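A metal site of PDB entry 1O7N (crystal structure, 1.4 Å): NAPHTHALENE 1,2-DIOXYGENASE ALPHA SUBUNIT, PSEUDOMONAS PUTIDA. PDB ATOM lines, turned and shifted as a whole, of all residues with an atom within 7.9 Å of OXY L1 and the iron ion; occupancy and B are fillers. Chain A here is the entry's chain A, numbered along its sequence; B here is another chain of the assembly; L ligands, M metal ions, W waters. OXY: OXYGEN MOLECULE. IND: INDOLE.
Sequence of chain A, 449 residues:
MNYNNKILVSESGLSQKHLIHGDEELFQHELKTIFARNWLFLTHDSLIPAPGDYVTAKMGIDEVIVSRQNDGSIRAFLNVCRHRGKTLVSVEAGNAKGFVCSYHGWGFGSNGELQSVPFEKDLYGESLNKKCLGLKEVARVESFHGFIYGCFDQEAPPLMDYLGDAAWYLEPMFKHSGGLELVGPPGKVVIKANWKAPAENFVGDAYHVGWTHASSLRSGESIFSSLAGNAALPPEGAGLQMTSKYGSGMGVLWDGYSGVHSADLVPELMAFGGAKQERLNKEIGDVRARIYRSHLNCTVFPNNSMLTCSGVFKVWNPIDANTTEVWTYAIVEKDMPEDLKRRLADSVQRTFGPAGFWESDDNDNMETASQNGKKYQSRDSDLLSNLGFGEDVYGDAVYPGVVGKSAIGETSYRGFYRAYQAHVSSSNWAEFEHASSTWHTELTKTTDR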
ATOM      1  N   PRO A 198     -12.808   2.687 -11.915  1.00  0.00           N
ATOM      2  CA  PRO A 198     -13.383   2.678 -13.267  1.00  0.00           C
ATOM      3  C   PRO A 198     -14.830   3.227 -13.282  1.00  0.00           C
ATOM      4  O   PRO A 198     -15.184   3.854 -14.292  1.00  0.00           O
ATOM      5  CB  PRO A 198     -13.290   1.228 -13.718  1.00  0.00           C
ATOM      6  CG  PRO A 198     -13.206   0.438 -12.415  1.00  0.00           C
ATOM      7  CD  PRO A 198     -12.427   1.328 -11.472  1.00  0.00           C
ATOM      8  N   ASN A 201     -14.594   6.903 -13.622  1.00  0.00           N
ATOM      9  CA  ASN A 201     -13.975   7.304 -14.885  1.00  0.00           C
ATOM     10  C   ASN A 201     -15.017   7.250 -15.986  1.00  0.00           C
ATOM     11  O   ASN A 201     -15.122   8.198 -16.797  1.00  0.00           O
ATOM     12  CB  ASN A 201     -12.794   6.372 -15.174  1.00  0.00           C
ATOM     13  CG  ASN A 201     -12.157   6.634 -16.517  1.00  0.00           C
ATOM     14  OD1 ASN A 201     -11.288   7.495 -16.626  1.00  0.00           O
ATOM     15  ND2 ASN A 201     -12.570   5.887 -17.517  1.00  0.00           N
ATOM     16  N   PHE A 202     -15.812   6.190 -16.045  1.00  0.00           N
ATOM     17  CA  PHE A 202     -16.879   6.093 -17.059  1.00  0.00           C
ATOM     18  C   PHE A 202     -18.047   7.030 -16.804  1.00  0.00           C
ATOM     19  O   PHE A 202     -18.642   7.513 -17.786  1.00  0.00           O
ATOM     20  CB  PHE A 202     -17.416   4.654 -17.231  1.00  0.00           C
ATOM     21  CG  PHE A 202     -16.554   3.794 -18.110  1.00  0.00           C
ATOM     22  CD1 PHE A 202     -15.251   3.466 -17.724  1.00  0.00           C
ATOM     23  CD2 PHE A 202     -17.042   3.256 -19.284  1.00  0.00           C
ATOM     24  CE1 PHE A 202     -14.458   2.667 -18.536  1.00  0.00           C
ATOM     25  CE2 PHE A 202     -16.230   2.433 -20.097  1.00  0.00           C
ATOM     26  CZ  PHE A 202     -14.930   2.162 -19.693  1.00  0.00           C
ATOM     27  N   ASP A 205     -15.660  11.163 -16.797  1.00  0.00           N
ATOM     28  CA  ASP A 205     -14.327  11.653 -17.057  1.00  0.00           C
ATOM     29  C   ASP A 205     -13.966  11.747 -18.533  1.00  0.00           C
ATOM     30  O   ASP A 205     -13.422  10.813 -19.120  1.00  0.00           O
ATOM     31  CB  ASP A 205     -13.343  10.758 -16.311  1.00  0.00           C
ATOM     32  CG  ASP A 205     -11.972  11.365 -16.213  1.00  0.00           C
ATOM     33  OD1 ASP A 205     -11.262  11.043 -15.240  1.00  0.00           O
ATOM     34  OD2 ASP A 205     -11.493  12.121 -17.074  1.00  0.00           O
ATOM     35  N   HIS A 208      -9.705  13.023 -19.085  1.00  0.00           N
ATOM     36  CA  HIS A 208      -8.538  12.134 -19.239  1.00  0.00           C
ATOM     37  C   HIS A 208      -8.314  11.669 -20.652  1.00  0.00           C
ATOM     38  O   HIS A 208      -7.234  11.204 -20.966  1.00  0.00           O
ATOM     39  CB  HIS A 208      -8.691  10.894 -18.315  1.00  0.00           C
ATOM     40  CG  HIS A 208      -9.455   9.764 -18.897  1.00  0.00           C
ATOM     41  ND1 HIS A 208     -10.822   9.793 -19.115  1.00  0.00           N
ATOM     42  CD2 HIS A 208      -9.052   8.537 -19.301  1.00  0.00           C
ATOM     43  CE1 HIS A 208     -11.210   8.642 -19.617  1.00  0.00           C
ATOM     44  NE2 HIS A 208     -10.158   7.854 -19.728  1.00  0.00           N
ATOM     45  N   VAL A 209      -9.327  11.724 -21.526  1.00  0.00           N
ATOM     46  CA  VAL A 209      -9.243  11.049 -22.814  1.00  0.00           C
ATOM     47  C   VAL A 209      -8.021  11.416 -23.676  1.00  0.00           C
ATOM     48  O   VAL A 209      -7.259  10.530 -24.096  1.00  0.00           O
ATOM     49  CB  VAL A 209     -10.590  11.172 -23.588  1.00  0.00           C
ATOM     50  CG1 VAL A 209     -10.457  10.606 -25.011  1.00  0.00           C
ATOM     51  CG2 VAL A 209     -11.669  10.411 -22.796  1.00  0.00           C
ATOM     52  N   THR A 212      -4.518  10.381 -21.285  1.00  0.00           N
ATOM     53  CA  THR A 212      -4.435   8.943 -21.039  1.00  0.00           C
ATOM     54  C   THR A 212      -4.431   8.142 -22.317  1.00  0.00           C
ATOM     55  O   THR A 212      -3.634   7.194 -22.489  1.00  0.00           O
ATOM     56  CB  THR A 212      -5.618   8.482 -20.179  1.00  0.00           C
ATOM     57  OG1 THR A 212      -5.493   8.961 -18.826  1.00  0.00           O
ATOM     58  CG2 THR A 212      -5.644   6.953 -20.062  1.00  0.00           C
ATOM     59  N   HIS A 213      -5.326   8.493 -23.247  1.00  0.00           N
ATOM     60  CA  HIS A 213      -5.497   7.708 -24.470  1.00  0.00           C
ATOM     61  C   HIS A 213      -4.766   8.262 -25.675  1.00  0.00           C
ATOM     62  O   HIS A 213      -5.058   7.847 -26.788  1.00  0.00           O
ATOM     63  CB  HIS A 213      -6.962   7.461 -24.798  1.00  0.00           C
ATOM     64  CG  HIS A 213      -7.686   6.679 -23.746  1.00  0.00           C
ATOM     65  ND1 HIS A 213      -7.401   5.357 -23.471  1.00  0.00           N
ATOM     66  CD2 HIS A 213      -8.678   7.030 -22.878  1.00  0.00           C
ATOM     67  CE1 HIS A 213      -8.172   4.927 -22.488  1.00  0.00           C
ATOM     68  NE2 HIS A 213      -8.970   5.916 -22.107  1.00  0.00           N
ATOM     69  N   VAL A 260     -15.079   4.953 -30.296  1.00  0.00           N
ATOM     70  CA  VAL A 260     -13.674   4.562 -30.265  1.00  0.00           C
ATOM     71  C   VAL A 260     -13.260   3.682 -31.449  1.00  0.00           C
ATOM     72  O   VAL A 260     -12.073   3.374 -31.620  1.00  0.00           O
ATOM     73  CB  VAL A 260     -13.386   3.823 -28.948  1.00  0.00           C
ATOM     74  CG1 VAL A 260     -13.861   4.673 -27.731  1.00  0.00           C
ATOM     75  CG2 VAL A 260     -14.076   2.466 -28.947  1.00  0.00           C
ATOM     76  N   ASN A 297     -21.014   8.243 -22.289  1.00  0.00           N
ATOM     77  CA  ASN A 297     -20.192   7.507 -21.379  1.00  0.00           C
ATOM     78  C   ASN A 297     -20.947   7.563 -20.078  1.00  0.00           C
ATOM     79  O   ASN A 297     -21.017   8.621 -19.447  1.00  0.00           O
ATOM     80  CB  ASN A 297     -18.756   8.052 -21.234  1.00  0.00           C
ATOM     81  CG  ASN A 297     -18.702   9.514 -20.871  1.00  0.00           C
ATOM     82  OD1 ASN A 297     -19.040  10.353 -21.694  1.00  0.00           O
ATOM     83  ND2 ASN A 297     -18.294   9.816 -19.639  1.00  0.00           N
ATOM     84  N   LEU A 307     -20.351   2.638 -22.879  1.00  0.00           N
ATOM     85  CA  LEU A 307     -20.120   3.685 -23.881  1.00  0.00           C
ATOM     86  C   LEU A 307     -21.099   3.369 -24.979  1.00  0.00           C
ATOM     87  O   LEU A 307     -20.894   2.392 -25.718  1.00  0.00           O
ATOM     88  CB  LEU A 307     -18.703   3.640 -24.449  1.00  0.00           C
ATOM     89  CG  LEU A 307     -17.574   3.765 -23.413  1.00  0.00           C
ATOM     90  CD1 LEU A 307     -16.202   3.703 -24.127  1.00  0.00           C
ATOM     91  CD2 LEU A 307     -17.691   5.043 -22.559  1.00  0.00           C
ATOM     92  N   LYS A 314     -19.789  -2.666 -19.457  1.00  0.00           N
ATOM     93  CA  LYS A 314     -18.904  -3.119 -18.384  1.00  0.00           C
ATOM     94  C   LYS A 314     -19.608  -3.370 -17.076  1.00  0.00           C
ATOM     95  O   LYS A 314     -20.514  -2.618 -16.678  1.00  0.00           O
ATOM     96  CB  LYS A 314     -17.898  -2.004 -18.065  1.00  0.00           C
ATOM     97  CG  LYS A 314     -16.947  -1.618 -19.174  1.00  0.00           C
ATOM     98  CD  LYS A 314     -15.759  -2.583 -19.222  1.00  0.00           C
ATOM     99  CE  LYS A 314     -14.723  -2.167 -20.286  1.00  0.00           C
ATOM    100  NZ  LYS A 314     -13.577  -3.195 -20.220  1.00  0.00           N
ATOM    101  N   TRP A 316     -18.148  -3.705 -13.126  1.00  0.00           N
ATOM    102  CA  TRP A 316     -16.969  -3.639 -12.273  1.00  0.00           C
ATOM    103  C   TRP A 316     -17.293  -4.435 -11.014  1.00  0.00           C
ATOM    104  O   TRP A 316     -17.750  -3.872 -10.014  1.00  0.00           O
ATOM    105  CB  TRP A 316     -16.665  -2.189 -11.910  1.00  0.00           C
ATOM    106  CG  TRP A 316     -16.757  -1.250 -13.056  1.00  0.00           C
ATOM    107  CD1 TRP A 316     -17.693  -0.248 -13.201  1.00  0.00           C
ATOM    108  CD2 TRP A 316     -15.864  -1.126 -14.195  1.00  0.00           C
ATOM    109  NE1 TRP A 316     -17.463   0.433 -14.374  1.00  0.00           N
ATOM    110  CE2 TRP A 316     -16.374  -0.083 -15.015  1.00  0.00           C
ATOM    111  CE3 TRP A 316     -14.736  -1.838 -14.639  1.00  0.00           C
ATOM    112  CZ2 TRP A 316     -15.772   0.304 -16.202  1.00  0.00           C
ATOM    113  CZ3 TRP A 316     -14.130  -1.439 -15.844  1.00  0.00           C
ATOM    114  CH2 TRP A 316     -14.667  -0.387 -16.607  1.00  0.00           C
ATOM    115  N   PHE A 352     -11.567  -2.279 -25.846  1.00  0.00           N
ATOM    116  CA  PHE A 352     -11.864  -2.255 -24.411  1.00  0.00           C
ATOM    117  C   PHE A 352     -11.948  -3.592 -23.740  1.00  0.00           C
ATOM    118  O   PHE A 352     -12.276  -3.635 -22.556  1.00  0.00           O
ATOM    119  CB  PHE A 352     -13.167  -1.438 -24.155  1.00  0.00           C
ATOM    120  CG  PHE A 352     -12.918   0.019 -24.112  1.00  0.00           C
ATOM    121  CD1 PHE A 352     -12.566   0.627 -22.929  1.00  0.00           C
ATOM    122  CD2 PHE A 352     -12.946   0.775 -25.259  1.00  0.00           C
ATOM    123  CE1 PHE A 352     -12.291   1.993 -22.885  1.00  0.00           C
ATOM    124  CE2 PHE A 352     -12.680   2.130 -25.214  1.00  0.00           C
ATOM    125  CZ  PHE A 352     -12.332   2.728 -24.067  1.00  0.00           C
ATOM    126  N   TRP A 358      -7.200   0.454 -25.731  1.00  0.00           N
ATOM    127  CA  TRP A 358      -7.606   1.661 -25.021  1.00  0.00           C
ATOM    128  C   TRP A 358      -7.699   1.356 -23.527  1.00  0.00           C
ATOM    129  O   TRP A 358      -7.198   2.134 -22.699  1.00  0.00           O
ATOM    130  CB  TRP A 358      -8.977   2.149 -25.485  1.00  0.00           C
ATOM    131  CG  TRP A 358      -9.059   2.742 -26.870  1.00  0.00           C
ATOM    132  CD1 TRP A 358      -8.815   2.115 -28.064  1.00  0.00           C
ATOM    133  CD2 TRP A 358      -9.500   4.053 -27.192  1.00  0.00           C
ATOM    134  NE1 TRP A 358      -9.061   2.976 -29.115  1.00  0.00           N
ATOM    135  CE2 TRP A 358      -9.489   4.162 -28.600  1.00  0.00           C
ATOM    136  CE3 TRP A 358      -9.919   5.151 -26.429  1.00  0.00           C
ATOM    137  CZ2 TRP A 358      -9.861   5.348 -29.262  1.00  0.00           C
ATOM    138  CZ3 TRP A 358     -10.300   6.326 -27.091  1.00  0.00           C
ATOM    139  CH2 TRP A 358     -10.265   6.410 -28.483  1.00  0.00           C
ATOM    140  N   GLU A 359      -8.347   0.247 -23.162  1.00  0.00           N
ATOM    141  CA  GLU A 359      -8.529  -0.097 -21.750  1.00  0.00           C
ATOM    142  C   GLU A 359      -7.169  -0.241 -21.072  1.00  0.00           C
ATOM    143  O   GLU A 359      -6.997   0.138 -19.893  1.00  0.00           O
ATOM    144  CB  GLU A 359      -9.342  -1.412 -21.651  1.00  0.00           C
ATOM    145  CG  GLU A 359      -9.548  -1.960 -20.230  1.00  0.00           C
ATOM    146  CD  GLU A 359     -10.945  -1.727 -19.677  1.00  0.00           C
ATOM    147  OE1 GLU A 359     -11.603  -0.736 -20.040  1.00  0.00           O
ATOM    148  OE2 GLU A 359     -11.399  -2.557 -18.825  1.00  0.00           O
ATOM    149  N   SER A 360      -6.181  -0.718 -21.820  1.00  0.00           N
ATOM    150  CA  SER A 360      -4.848  -0.855 -21.265  1.00  0.00           C
ATOM    151  C   SER A 360      -4.262   0.485 -20.829  1.00  0.00           C
ATOM    152  O   SER A 360      -3.530   0.540 -19.847  1.00  0.00           O
ATOM    153  CB  SER A 360      -3.916  -1.568 -22.275  1.00  0.00           C
ATOM    154  OG  SER A 360      -3.398  -0.674 -23.241  1.00  0.00           O
ATOM    155  N   ASP A 361      -4.604   1.565 -21.518  1.00  0.00           N
ATOM    156  CA  ASP A 361      -4.062   2.885 -21.174  1.00  0.00           C
ATOM    157  C   ASP A 361      -4.549   3.325 -19.787  1.00  0.00           C
ATOM    158  O   ASP A 361      -3.886   4.164 -19.142  1.00  0.00           O
ATOM    159  CB  ASP A 361      -4.588   3.969 -22.142  1.00  0.00           C
ATOM    160  CG  ASP A 361      -4.257   3.747 -23.601  1.00  0.00           C
ATOM    161  OD1 ASP A 361      -5.017   4.235 -24.464  1.00  0.00           O
ATOM    162  OD2 ASP A 361      -3.235   3.124 -23.963  1.00  0.00           O
ATOM    163  N   ASP A 362      -5.724   2.838 -19.372  1.00  0.00           N
ATOM    164  CA  ASP A 362      -6.327   3.248 -18.089  1.00  0.00           C
ATOM    165  C   ASP A 362      -5.818   2.431 -16.919  1.00  0.00           C
ATOM    166  O   ASP A 362      -6.024   2.852 -15.781  1.00  0.00           O
ATOM    167  CB  ASP A 362      -7.846   3.039 -18.109  1.00  0.00           C
ATOM    168  CG  ASP A 362      -8.573   3.988 -19.017  1.00  0.00           C
ATOM    169  OD1 ASP A 362      -9.242   3.524 -19.952  1.00  0.00           O
ATOM    170  OD2 ASP A 362      -8.596   5.190 -18.800  1.00  0.00           O
ATOM    171  N   ASN A 363      -5.183   1.270 -17.146  1.00  0.00           N
ATOM    172  CA  ASN A 363      -4.809   0.345 -16.035  1.00  0.00           C
ATOM    173  C   ASN A 363      -4.034   0.997 -14.923  1.00  0.00           C
ATOM    174  O   ASN A 363      -4.409   0.891 -13.745  1.00  0.00           O
ATOM    175  CB  ASN A 363      -3.890  -0.801 -16.515  1.00  0.00           C
ATOM    176  CG  ASN A 363      -4.620  -1.919 -17.237  1.00  0.00           C
ATOM    177  OD1 ASN A 363      -3.969  -2.816 -17.808  1.00  0.00           O
ATOM    178  ND2 ASN A 363      -5.971  -1.918 -17.185  1.00  0.00           N
ATOM    179  N   ASN A 365      -3.552   4.072 -14.202  1.00  0.00           N
ATOM    180  CA  ASN A 365      -4.267   5.160 -13.557  1.00  0.00           C
ATOM    181  C   ASN A 365      -5.200   4.612 -12.487  1.00  0.00           C
ATOM    182  O   ASN A 365      -5.170   5.094 -11.360  1.00  0.00           O
ATOM    183  CB  ASN A 365      -5.067   5.994 -14.559  1.00  0.00           C
ATOM    184  CG  ASN A 365      -4.172   6.741 -15.543  1.00  0.00           C
ATOM    185  OD1 ASN A 365      -2.994   7.022 -15.275  1.00  0.00           O
ATOM    186  ND2 ASN A 365      -4.740   7.069 -16.693  1.00  0.00           N
ATOM    187  N   MET A 366      -6.003   3.617 -12.832  1.00  0.00           N
ATOM    188  CA  MET A 366      -6.928   3.078 -11.867  1.00  0.00           C
ATOM    189  C   MET A 366      -6.253   2.239 -10.806  1.00  0.00           C
ATOM    190  O   MET A 366      -6.653   2.340  -9.630  1.00  0.00           O
ATOM    191  CB  MET A 366      -8.033   2.318 -12.585  1.00  0.00           C
ATOM    192  CG  MET A 366      -8.547   2.620 -13.844  1.00  0.00           C
ATOM    193  SD  MET A 366      -9.872   3.698 -13.475  1.00  0.00           S
ATOM    194  CE  MET A 366      -9.045   5.246 -13.554  1.00  0.00           C
ATOM    195  N   TYR B 103      -2.661  10.678 -16.036  1.00  0.00           N
ATOM    196  CA  TYR B 103      -4.125  10.557 -16.008  1.00  0.00           C
ATOM    197  C   TYR B 103      -4.801  11.755 -16.729  1.00  0.00           C
ATOM    198  O   TYR B 103      -5.387  11.589 -17.795  1.00  0.00           O
ATOM    199  CB  TYR B 103      -4.626  10.388 -14.573  1.00  0.00           C
ATOM    200  CG  TYR B 103      -5.984   9.720 -14.398  1.00  0.00           C
ATOM    201  CD1 TYR B 103      -6.390   9.243 -13.160  1.00  0.00           C
ATOM    202  CD2 TYR B 103      -6.847   9.542 -15.466  1.00  0.00           C
ATOM    203  CE1 TYR B 103      -7.659   8.686 -12.980  1.00  0.00           C
ATOM    204  CE2 TYR B 103      -8.111   8.989 -15.298  1.00  0.00           C
ATOM    205  CZ  TYR B 103      -8.510   8.560 -14.058  1.00  0.00           C
ATOM    206  OH  TYR B 103      -9.752   8.000 -13.886  1.00  0.00           O
HETATM  207  O1  OXY L   1     -11.409   5.645 -21.257  1.00  0.00           O
HETATM  208  O2  OXY L   1     -11.783   5.021 -19.996  1.00  0.00           O
HETATM  209  N1  IND L   2     -15.016   8.005 -20.106  1.00  0.00           N
HETATM  210  C2  IND L   2     -14.396   6.774 -20.173  1.00  0.00           C
HETATM  211  C3  IND L   2     -14.067   6.393 -21.468  1.00  0.00           C
HETATM  212  C4  IND L   2     -14.481   7.679 -23.590  1.00  0.00           C
HETATM  213  C5  IND L   2     -15.027   8.850 -24.128  1.00  0.00           C
HETATM  214  C6  IND L   2     -15.598   9.822 -23.294  1.00  0.00           C
HETATM  215  C7  IND L   2     -15.666   9.674 -21.911  1.00  0.00           C
HETATM  216  C8  IND L   2     -15.148   8.526 -21.351  1.00  0.00           C
HETATM  217  C9  IND L   2     -14.540   7.513 -22.218  1.00  0.00           C
HETATM  218 FE    FE M   1      -9.976   5.779 -20.305  1.00  0.00          FE
HETATM  219  O   HOH W   1     -11.190   1.901 -19.232  1.00  0.00           O
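The iron ion is bound by an oxygen (O1) of OXY L1, 1.7 Å away. A ring nitrogen (NE2) of His 213 is bound to the iron ion, at 2.1 Å. The side-chain carboxylate (OD2) of Asp 362 is bound to the iron ion, at 2.1 Å. The iron ion is bound by NE2 of His 208 (2.2 Å). OD1 of Asp 362 is bound to the iron ion, at 2.4 Å. The iron ion has five donor atoms within binding distance.
The side-chain amide nitrogen of Asn 201 sits close to an oxygen (O2) of OXY L1 (2.7 Å). O of Asn 201 sits at hydrogen-bond distance from N1 of IND L2, at 3.3 Å. The backbone carbonyl oxygen (O) of Asp 205 sits at hydrogen-bond distance from a nitrogen (N1) of IND L2 (3.4 Å).
Phe 202 touches OXY L1. Hydrophobic or aromatic side chains that line OXY L1: Phe 202, His 208 and His 213. Of the 23 residues printed, 5 come within 4 Å of OXY L1.
Asn 201 touches the iron ion. Of the 23 residues printed, 4 come within 4 Å of the iron ion. The nearest printed residue that does not touch the iron ion is Thr 212 (4.5 Å).
O of Trp 358 sits close to ND1 of His 213, 3.3 Å away. ND1 of His 213 lies within hydrogen-bond range of OD1 of Asp 361 (2.8 Å). ND1 of His 208 sits close to OD1 of Asn 201 (3.4 Å). A ring nitrogen (ND1) of His 208 is in hydrogen-bond range of the backbone carbonyl oxygen of Asp 205, 2.8 Å away. The side-chain amide oxygen (OD1) of Asn 201 lies within hydrogen-bond range of the side-chain hydroxyl (OH) of Tyr 103 of chain B (3.2 Å). ND2 of Asn 297 lies within hydrogen-bond range of O of Phe 202, 3.0 Å away.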
